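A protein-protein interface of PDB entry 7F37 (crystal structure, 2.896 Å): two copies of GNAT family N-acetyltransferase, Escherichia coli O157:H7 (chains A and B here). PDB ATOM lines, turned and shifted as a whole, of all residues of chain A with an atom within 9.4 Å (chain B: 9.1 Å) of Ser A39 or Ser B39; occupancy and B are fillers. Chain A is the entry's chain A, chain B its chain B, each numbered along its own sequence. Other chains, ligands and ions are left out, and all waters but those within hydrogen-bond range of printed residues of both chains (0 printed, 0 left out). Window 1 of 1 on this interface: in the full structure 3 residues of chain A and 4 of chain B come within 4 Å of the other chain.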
ATOM      1  N   LYS A  31      21.840 -16.837 -25.435  1.00  0.00           N
ATOM      2  CA  LYS A  31      21.048 -17.922 -25.992  1.00  0.00           C
ATOM      3  C   LYS A  31      20.836 -19.063 -25.004  1.00  0.00           C
ATOM      4  O   LYS A  31      19.692 -19.350 -24.638  1.00  0.00           O
ATOM      5  CB  LYS A  31      21.708 -18.413 -27.294  1.00  0.00           C
ATOM      6  CG  LYS A  31      21.725 -17.341 -28.412  1.00  0.00           C
ATOM      7  CD  LYS A  31      21.939 -17.956 -29.791  1.00  0.00           C
ATOM      8  CE  LYS A  31      21.065 -19.199 -30.031  1.00  0.00           C
ATOM      9  NZ  LYS A  31      21.538 -20.072 -31.164  1.00  0.00           N
ATOM     10  N   LYS A  32      21.902 -19.676 -24.492  1.00  0.00           N
ATOM     11  CA  LYS A  32      21.780 -20.959 -23.806  1.00  0.00           C
ATOM     12  C   LYS A  32      21.771 -20.878 -22.269  1.00  0.00           C
ATOM     13  O   LYS A  32      21.547 -21.897 -21.622  1.00  0.00           O
ATOM     14  CB  LYS A  32      22.900 -21.896 -24.292  1.00  0.00           C
ATOM     15  CG  LYS A  32      22.863 -22.116 -25.817  1.00  0.00           C
ATOM     16  CD  LYS A  32      23.786 -23.258 -26.288  1.00  0.00           C
ATOM     17  CE  LYS A  32      23.641 -23.550 -27.796  1.00  0.00           C
ATOM     18  NZ  LYS A  32      24.929 -23.941 -28.470  1.00  0.00           N
ATOM     19  N   ALA A  33      21.952 -19.699 -21.667  1.00  0.00           N
ATOM     20  CA  ALA A  33      22.121 -19.628 -20.216  1.00  0.00           C
ATOM     21  C   ALA A  33      20.834 -19.956 -19.472  1.00  0.00           C
ATOM     22  O   ALA A  33      20.801 -20.871 -18.644  1.00  0.00           O
ATOM     23  CB  ALA A  33      22.617 -18.246 -19.806  1.00  0.00           C
ATOM     24  N   LEU A  34      19.767 -19.195 -19.722  1.00  0.00           N
ATOM     25  CA  LEU A  34      18.560 -19.375 -18.920  1.00  0.00           C
ATOM     26  C   LEU A  34      17.863 -20.702 -19.232  1.00  0.00           C
ATOM     27  O   LEU A  34      17.386 -21.378 -18.315  1.00  0.00           O
ATOM     28  CB  LEU A  34      17.614 -18.189 -19.120  1.00  0.00           C
ATOM     29  CG  LEU A  34      16.310 -18.183 -18.304  1.00  0.00           C
ATOM     30  CD1 LEU A  34      16.560 -18.373 -16.816  1.00  0.00           C
ATOM     31  CD2 LEU A  34      15.514 -16.921 -18.543  1.00  0.00           C
ATOM     32  N   LYS A  35      17.796 -21.102 -20.511  1.00  0.00           N
ATOM     33  CA  LYS A  35      17.212 -22.403 -20.838  1.00  0.00           C
ATOM     34  C   LYS A  35      18.036 -23.541 -20.240  1.00  0.00           C
ATOM     35  O   LYS A  35      17.485 -24.570 -19.829  1.00  0.00           O
ATOM     36  CB  LYS A  35      17.077 -22.571 -22.360  1.00  0.00           C
ATOM     37  CG  LYS A  35      16.404 -23.881 -22.824  1.00  0.00           C
ATOM     38  CD  LYS A  35      16.048 -23.884 -24.332  1.00  0.00           C
ATOM     39  CE  LYS A  35      17.290 -23.978 -25.246  1.00  0.00           C
ATOM     40  NZ  LYS A  35      17.009 -24.174 -26.719  1.00  0.00           N
ATOM     41  N   ASN A  36      19.363 -23.378 -20.193  1.00  0.00           N
ATOM     42  CA  ASN A  36      20.220 -24.369 -19.548  1.00  0.00           C
ATOM     43  C   ASN A  36      20.000 -24.386 -18.043  1.00  0.00           C
ATOM     44  O   ASN A  36      19.753 -25.442 -17.450  1.00  0.00           O
ATOM     45  CB  ASN A  36      21.690 -24.076 -19.845  1.00  0.00           C
ATOM     46  CG  ASN A  36      22.416 -25.268 -20.384  1.00  0.00           C
ATOM     47  OD1 ASN A  36      21.885 -25.997 -21.223  1.00  0.00           O
ATOM     48  ND2 ASN A  36      23.643 -25.482 -19.906  1.00  0.00           N
ATOM     49  N   HIS A  37      20.108 -23.214 -17.409  1.00  0.00           N
ATOM     50  CA  HIS A  37      20.009 -23.118 -15.957  1.00  0.00           C
ATOM     51  C   HIS A  37      18.645 -23.605 -15.439  1.00  0.00           C
ATOM     52  O   HIS A  37      18.567 -24.255 -14.383  1.00  0.00           O
ATOM     53  CB  HIS A  37      20.311 -21.672 -15.543  1.00  0.00           C
ATOM     54  CG  HIS A  37      20.025 -21.386 -14.112  1.00  0.00           C
ATOM     55  ND1 HIS A  37      19.315 -20.280 -13.707  1.00  0.00           N
ATOM     56  CD2 HIS A  37      20.336 -22.069 -12.989  1.00  0.00           C
ATOM     57  CE1 HIS A  37      19.199 -20.294 -12.392  1.00  0.00           C
ATOM     58  NE2 HIS A  37      19.808 -21.372 -11.932  1.00  0.00           N
ATOM     59  N   SER A  38      17.573 -23.349 -16.196  1.00  0.00           N
ATOM     60  CA  SER A  38      16.230 -23.749 -15.789  1.00  0.00           C
ATOM     61  C   SER A  38      15.995 -25.234 -15.962  1.00  0.00           C
ATOM     62  O   SER A  38      15.246 -25.828 -15.175  1.00  0.00           O
ATOM     63  CB  SER A  38      15.180 -22.993 -16.600  1.00  0.00           C
ATOM     64  OG  SER A  38      15.302 -23.296 -17.982  1.00  0.00           O
ATOM     65  N   SER A  39      16.586 -25.834 -17.002  1.00  0.00           N
ATOM     66  CA  SER A  39      16.469 -27.272 -17.207  1.00  0.00           C
ATOM     67  C   SER A  39      17.423 -28.055 -16.323  1.00  0.00           C
ATOM     68  O   SER A  39      17.344 -29.286 -16.311  1.00  0.00           O
ATOM     69  CB  SER A  39      16.684 -27.633 -18.683  1.00  0.00           C
ATOM     70  OG  SER A  39      18.036 -27.893 -18.985  1.00  0.00           O
ATOM     71  N   GLY A  40      18.313 -27.366 -15.598  1.00  0.00           N
ATOM     72  CA  GLY A  40      19.046 -27.930 -14.476  1.00  0.00           C
ATOM     73  C   GLY A  40      20.391 -28.555 -14.780  1.00  0.00           C
ATOM     74  O   GLY A  40      20.973 -29.180 -13.883  1.00  0.00           O
ATOM     75  N   LEU A  41      20.915 -28.398 -16.000  1.00  0.00           N
ATOM     76  CA  LEU A  41      22.203 -28.996 -16.345  1.00  0.00           C
ATOM     77  C   LEU A  41      23.388 -28.299 -15.658  1.00  0.00           C
ATOM     78  O   LEU A  41      24.063 -28.900 -14.805  1.00  0.00           O
ATOM     79  CB  LEU A  41      22.365 -28.983 -17.863  1.00  0.00           C
ATOM     80  CG  LEU A  41      21.204 -29.653 -18.609  1.00  0.00           C
ATOM     81  CD1 LEU A  41      20.886 -28.890 -19.904  1.00  0.00           C
ATOM     82  CD2 LEU A  41      21.459 -31.165 -18.883  1.00  0.00           C
ATOM     83  N   SER A  42      23.630 -27.027 -15.993  1.00  0.00           N
ATOM     84  CA  SER A  42      24.534 -26.170 -15.233  1.00  0.00           C
ATOM     85  C   SER A  42      23.731 -25.099 -14.491  1.00  0.00           C
ATOM     86  O   SER A  42      22.589 -24.804 -14.843  1.00  0.00           O
ATOM     87  CB  SER A  42      25.618 -25.544 -16.147  1.00  0.00           C
ATOM     88  OG  SER A  42      25.182 -24.445 -16.943  1.00  0.00           O
ATOM     89  N   ARG A  43      24.332 -24.532 -13.440  1.00  0.00           N
ATOM     90  CA  ARG A  43      23.716 -23.486 -12.625  1.00  0.00           C
ATOM     91  C   ARG A  43      24.478 -22.159 -12.773  1.00  0.00           C
ATOM     92  O   ARG A  43      25.707 -22.128 -12.666  1.00  0.00           O
ATOM     93  CB  ARG A  43      23.666 -23.942 -11.174  1.00  0.00           C
ATOM     94  CG  ARG A  43      23.511 -22.847 -10.187  1.00  0.00           C
ATOM     95  CD  ARG A  43      22.057 -22.506  -9.931  1.00  0.00           C
ATOM     96  NE  ARG A  43      21.407 -23.525  -9.125  1.00  0.00           N
ATOM     97  CZ  ARG A  43      20.380 -24.249  -9.551  1.00  0.00           C
ATOM     98  NH1 ARG A  43      19.897 -24.046 -10.776  1.00  0.00           N
ATOM     99  NH2 ARG A  43      19.844 -25.179  -8.757  1.00  0.00           N
ATOM    100  N   VAL A  44      23.756 -21.066 -13.020  1.00  0.00           N
ATOM    101  CA  VAL A  44      24.345 -19.833 -13.537  1.00  0.00           C
ATOM    102  C   VAL A  44      24.063 -18.679 -12.573  1.00  0.00           C
ATOM    103  O   VAL A  44      22.913 -18.481 -12.161  1.00  0.00           O
ATOM    104  CB  VAL A  44      23.796 -19.513 -14.939  1.00  0.00           C
ATOM    105  CG1 VAL A  44      24.305 -18.166 -15.459  1.00  0.00           C
ATOM    106  CG2 VAL A  44      24.139 -20.624 -15.906  1.00  0.00           C
ATOM    107  N   LYS B  31      12.445 -39.253 -17.693  1.00  0.00           N
ATOM    108  CA  LYS B  31      13.836 -38.901 -17.898  1.00  0.00           C
ATOM    109  C   LYS B  31      14.044 -37.612 -18.661  1.00  0.00           C
ATOM    110  O   LYS B  31      15.086 -36.983 -18.470  1.00  0.00           O
ATOM    111  CB  LYS B  31      14.576 -40.039 -18.619  1.00  0.00           C
ATOM    112  CG  LYS B  31      14.375 -41.443 -17.984  1.00  0.00           C
ATOM    113  CD  LYS B  31      15.604 -41.921 -17.200  1.00  0.00           C
ATOM    114  CE  LYS B  31      15.425 -43.329 -16.664  1.00  0.00           C
ATOM    115  NZ  LYS B  31      16.631 -43.815 -15.923  1.00  0.00           N
ATOM    116  N   LYS B  32      13.097 -37.176 -19.483  1.00  0.00           N
ATOM    117  CA  LYS B  32      13.301 -36.007 -20.330  1.00  0.00           C
ATOM    118  C   LYS B  32      12.120 -35.045 -20.362  1.00  0.00           C
ATOM    119  O   LYS B  32      12.213 -34.015 -21.037  1.00  0.00           O
ATOM    120  CB  LYS B  32      13.627 -36.452 -21.766  1.00  0.00           C
ATOM    121  CG  LYS B  32      14.975 -37.090 -21.873  1.00  0.00           C
ATOM    122  CD  LYS B  32      15.299 -37.482 -23.282  1.00  0.00           C
ATOM    123  CE  LYS B  32      16.537 -38.374 -23.310  1.00  0.00           C
ATOM    124  NZ  LYS B  32      16.401 -39.578 -22.438  1.00  0.00           N
ATOM    125  N   ALA B  33      11.024 -35.343 -19.662  1.00  0.00           N
ATOM    126  CA  ALA B  33       9.792 -34.582 -19.807  1.00  0.00           C
ATOM    127  C   ALA B  33       9.843 -33.280 -19.025  1.00  0.00           C
ATOM    128  O   ALA B  33       9.444 -32.224 -19.534  1.00  0.00           O
ATOM    129  CB  ALA B  33       8.609 -35.425 -19.356  1.00  0.00           C
ATOM    130  N   LEU B  34      10.317 -33.329 -17.777  1.00  0.00           N
ATOM    131  CA  LEU B  34      10.510 -32.079 -17.055  1.00  0.00           C
ATOM    132  C   LEU B  34      11.816 -31.395 -17.436  1.00  0.00           C
ATOM    133  O   LEU B  34      11.948 -30.186 -17.234  1.00  0.00           O
ATOM    134  CB  LEU B  34      10.447 -32.300 -15.537  1.00  0.00           C
ATOM    135  CG  LEU B  34      10.071 -31.042 -14.717  1.00  0.00           C
ATOM    136  CD1 LEU B  34       8.916 -30.280 -15.357  1.00  0.00           C
ATOM    137  CD2 LEU B  34       9.736 -31.355 -13.260  1.00  0.00           C
ATOM    138  N   LYS B  35      12.783 -32.122 -17.985  1.00  0.00           N
ATOM    139  CA  LYS B  35      13.981 -31.441 -18.466  1.00  0.00           C
ATOM    140  C   LYS B  35      13.650 -30.624 -19.711  1.00  0.00           C
ATOM    141  O   LYS B  35      14.165 -29.511 -19.899  1.00  0.00           O
ATOM    142  CB  LYS B  35      15.092 -32.468 -18.733  1.00  0.00           C
ATOM    143  CG  LYS B  35      16.403 -31.926 -19.256  1.00  0.00           C
ATOM    144  CD  LYS B  35      16.881 -32.735 -20.478  1.00  0.00           C
ATOM    145  CE  LYS B  35      17.666 -31.879 -21.512  1.00  0.00           C
ATOM    146  NZ  LYS B  35      16.800 -31.070 -22.446  1.00  0.00           N
ATOM    147  N   ASN B  36      12.747 -31.153 -20.547  1.00  0.00           N
ATOM    148  CA  ASN B  36      12.320 -30.489 -21.772  1.00  0.00           C
ATOM    149  C   ASN B  36      11.288 -29.409 -21.489  1.00  0.00           C
ATOM    150  O   ASN B  36      11.441 -28.269 -21.937  1.00  0.00           O
ATOM    151  CB  ASN B  36      11.740 -31.508 -22.750  1.00  0.00           C
ATOM    152  CG  ASN B  36      12.786 -32.137 -23.630  1.00  0.00           C
ATOM    153  OD1 ASN B  36      13.990 -31.940 -23.452  1.00  0.00           O
ATOM    154  ND2 ASN B  36      12.324 -32.905 -24.606  1.00  0.00           N
ATOM    155  N   HIS B  37      10.225 -29.749 -20.750  1.00  0.00           N
ATOM    156  CA  HIS B  37       9.116 -28.814 -20.568  1.00  0.00           C
ATOM    157  C   HIS B  37       9.522 -27.573 -19.765  1.00  0.00           C
ATOM    158  O   HIS B  37       8.985 -26.479 -20.002  1.00  0.00           O
ATOM    159  CB  HIS B  37       7.967 -29.557 -19.909  1.00  0.00           C
ATOM    160  CG  HIS B  37       6.847 -28.685 -19.455  1.00  0.00           C
ATOM    161  ND1 HIS B  37       6.489 -28.571 -18.131  1.00  0.00           N
ATOM    162  CD2 HIS B  37       5.971 -27.930 -20.148  1.00  0.00           C
ATOM    163  CE1 HIS B  37       5.452 -27.762 -18.025  1.00  0.00           C
ATOM    164  NE2 HIS B  37       5.122 -27.355 -19.234  1.00  0.00           N
ATOM    165  N   SER B  38      10.489 -27.719 -18.838  1.00  0.00           N
ATOM    166  CA  SER B  38      11.009 -26.590 -18.057  1.00  0.00           C
ATOM    167  C   SER B  38      11.926 -25.689 -18.877  1.00  0.00           C
ATOM    168  O   SER B  38      12.075 -24.501 -18.551  1.00  0.00           O
ATOM    169  CB  SER B  38      11.784 -27.090 -16.840  1.00  0.00           C
ATOM    170  OG  SER B  38      10.966 -27.877 -16.002  1.00  0.00           O
ATOM    171  N   SER B  39      12.586 -26.251 -19.902  1.00  0.00           N
ATOM    172  CA  SER B  39      13.396 -25.489 -20.845  1.00  0.00           C
ATOM    173  C   SER B  39      12.623 -25.099 -22.102  1.00  0.00           C
ATOM    174  O   SER B  39      13.233 -24.963 -23.175  1.00  0.00           O
ATOM    175  CB  SER B  39      14.663 -26.270 -21.212  1.00  0.00           C
ATOM    176  OG  SER B  39      14.381 -27.606 -21.594  1.00  0.00           O
ATOM    177  N   GLY B  40      11.290 -24.953 -21.998  1.00  0.00           N
ATOM    178  CA  GLY B  40      10.414 -24.423 -23.042  1.00  0.00           C
ATOM    179  C   GLY B  40      10.626 -24.934 -24.453  1.00  0.00           C
ATOM    180  O   GLY B  40      10.217 -24.280 -25.419  1.00  0.00           O
ATOM    181  N   LEU B  41      11.251 -26.110 -24.580  1.00  0.00           N
ATOM    182  CA  LEU B  41      11.436 -26.750 -25.881  1.00  0.00           C
ATOM    183  C   LEU B  41      10.106 -27.316 -26.361  1.00  0.00           C
ATOM    184  O   LEU B  41       9.533 -26.846 -27.351  1.00  0.00           O
ATOM    185  CB  LEU B  41      12.482 -27.867 -25.779  1.00  0.00           C
ATOM    186  CG  LEU B  41      13.992 -27.635 -25.683  1.00  0.00           C
ATOM    187  CD1 LEU B  41      14.730 -28.931 -26.056  1.00  0.00           C
ATOM    188  CD2 LEU B  41      14.424 -26.481 -26.574  1.00  0.00           C
ATOM    189  N   SER B  42       9.594 -28.311 -25.636  1.00  0.00           N
ATOM    190  CA  SER B  42       8.245 -28.830 -25.783  1.00  0.00           C
ATOM    191  C   SER B  42       7.413 -28.404 -24.575  1.00  0.00           C
ATOM    192  O   SER B  42       7.863 -27.674 -23.687  1.00  0.00           O
ATOM    193  CB  SER B  42       8.271 -30.347 -25.935  1.00  0.00           C
ATOM    194  OG  SER B  42       9.074 -30.937 -24.933  1.00  0.00           O
ATOM    195  N   ARG B  43       6.176 -28.864 -24.531  1.00  0.00           N
ATOM    196  CA  ARG B  43       5.269 -28.454 -23.472  1.00  0.00           C
ATOM    197  C   ARG B  43       4.419 -29.664 -23.119  1.00  0.00           C
ATOM    198  O   ARG B  43       3.645 -30.130 -23.961  1.00  0.00           O
ATOM    199  CB  ARG B  43       4.440 -27.275 -23.946  1.00  0.00           C
ATOM    200  CG  ARG B  43       3.281 -26.898 -23.087  1.00  0.00           C
ATOM    201  CD  ARG B  43       3.702 -26.299 -21.755  1.00  0.00           C
ATOM    202  NE  ARG B  43       3.688 -24.844 -21.711  1.00  0.00           N
ATOM    203  CZ  ARG B  43       4.655 -24.118 -21.161  1.00  0.00           C
ATOM    204  NH1 ARG B  43       5.704 -24.727 -20.612  1.00  0.00           N
ATOM    205  NH2 ARG B  43       4.578 -22.785 -21.161  1.00  0.00           N
ATOM    206  N   VAL B  44       4.577 -30.200 -21.892  1.00  0.00           N
ATOM    207  CA  VAL B  44       3.993 -31.495 -21.524  1.00  0.00           C
ATOM    208  C   VAL B  44       2.699 -31.298 -20.721  1.00  0.00           C
ATOM    209  O   VAL B  44       2.583 -30.367 -19.919  1.00  0.00           O
ATOM    210  CB  VAL B  44       5.034 -32.340 -20.761  1.00  0.00           C
ATOM    211  CG1 VAL B  44       4.498 -33.702 -20.426  1.00  0.00           C
ATOM    212  CG2 VAL B  44       6.284 -32.495 -21.600  1.00  0.00           C
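The side-chain hydroxyl of Ser A38 lies within hydrogen-bond range of the backbone carbonyl oxygen of Ser B38 (3.5 Å).
The side-chain amide oxygen (OD1) of Asn B36 is in hydrogen-bond range of the side-chain amino group (NZ) of Lys B35. The backbone carbonyl oxygen (O) of Asn A36 sits at hydrogen-bond distance from the side-chain hydroxyl (OG) of Ser A39, at 3.4 Å. The backbone carbonyl oxygen (O) of Lys B35 lies within hydrogen-bond range of the side-chain hydroxyl (OG) of Ser B39 (2.6 Å). OG of Ser A39 sits close to O of Lys A35 (3.5 Å). O of Asn B36 lies within hydrogen-bond range of OG of Ser B39. O of Asn B36 sits at hydrogen-bond distance from N of Leu B41 (3.4 Å).
Among the printed residues, pairs that only touch across the chains: Lys A35 with Ser B39 (3.2 Å), Lys A35 with Leu B41 (3.5 Å), Ser A39 with Lys B35 (3.4 Å) and Ser A39 with Ser B39 (3.5 Å).
Lys A31 touches none of the printed residues of chain B. Printed residues of chain B within 4 Å of Lys A35: Ser B39 and Leu B41. Of chain B, only Ser B38 (3.5 Å) comes within 4 Å of Ser A38. Gly A40 touches none of the printed residues of chain B. Of the printed residues of chain A, Lys B35 touches Ser A39. Of the printed residues of chain A, Ser B38 touches Ser A38. Of the printed residues of chain A, Ser B39 touches Lys A35 and Ser A39. Printed residues of chain A within 4 Å of Leu B41: Lys A35. The nearest residue of chain B that does not touch Ser A39 is Ser B38 (4.7 Å). The nearest printed residue of chain B that does not touch Lys A35 is Gly B40 (5.3 Å).
Of the 14 printed residues of chain B, 4 touch a printed residue of chain A. Along chain B the printed residues that touch a printed residue of chain A span positions 35 to 41. Among the printed residues, 5 pairs touch across the chains. Among the printed residues, no Asp or Glu carboxylate lies within 4 Å of a Lys or Arg side-chain nitrogen of the other chain.
Lys A35 touches Ser B39, and with the chains exchanged Ser A39 touches Lys B35. Lys A35 touches Leu B41, but with the chains exchanged Leu A41 does not touch Lys B35 (4.7 Å). Ser B38 touches its own counterpart, Ser A38. Ser A39 touches its own counterpart, Ser B39.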
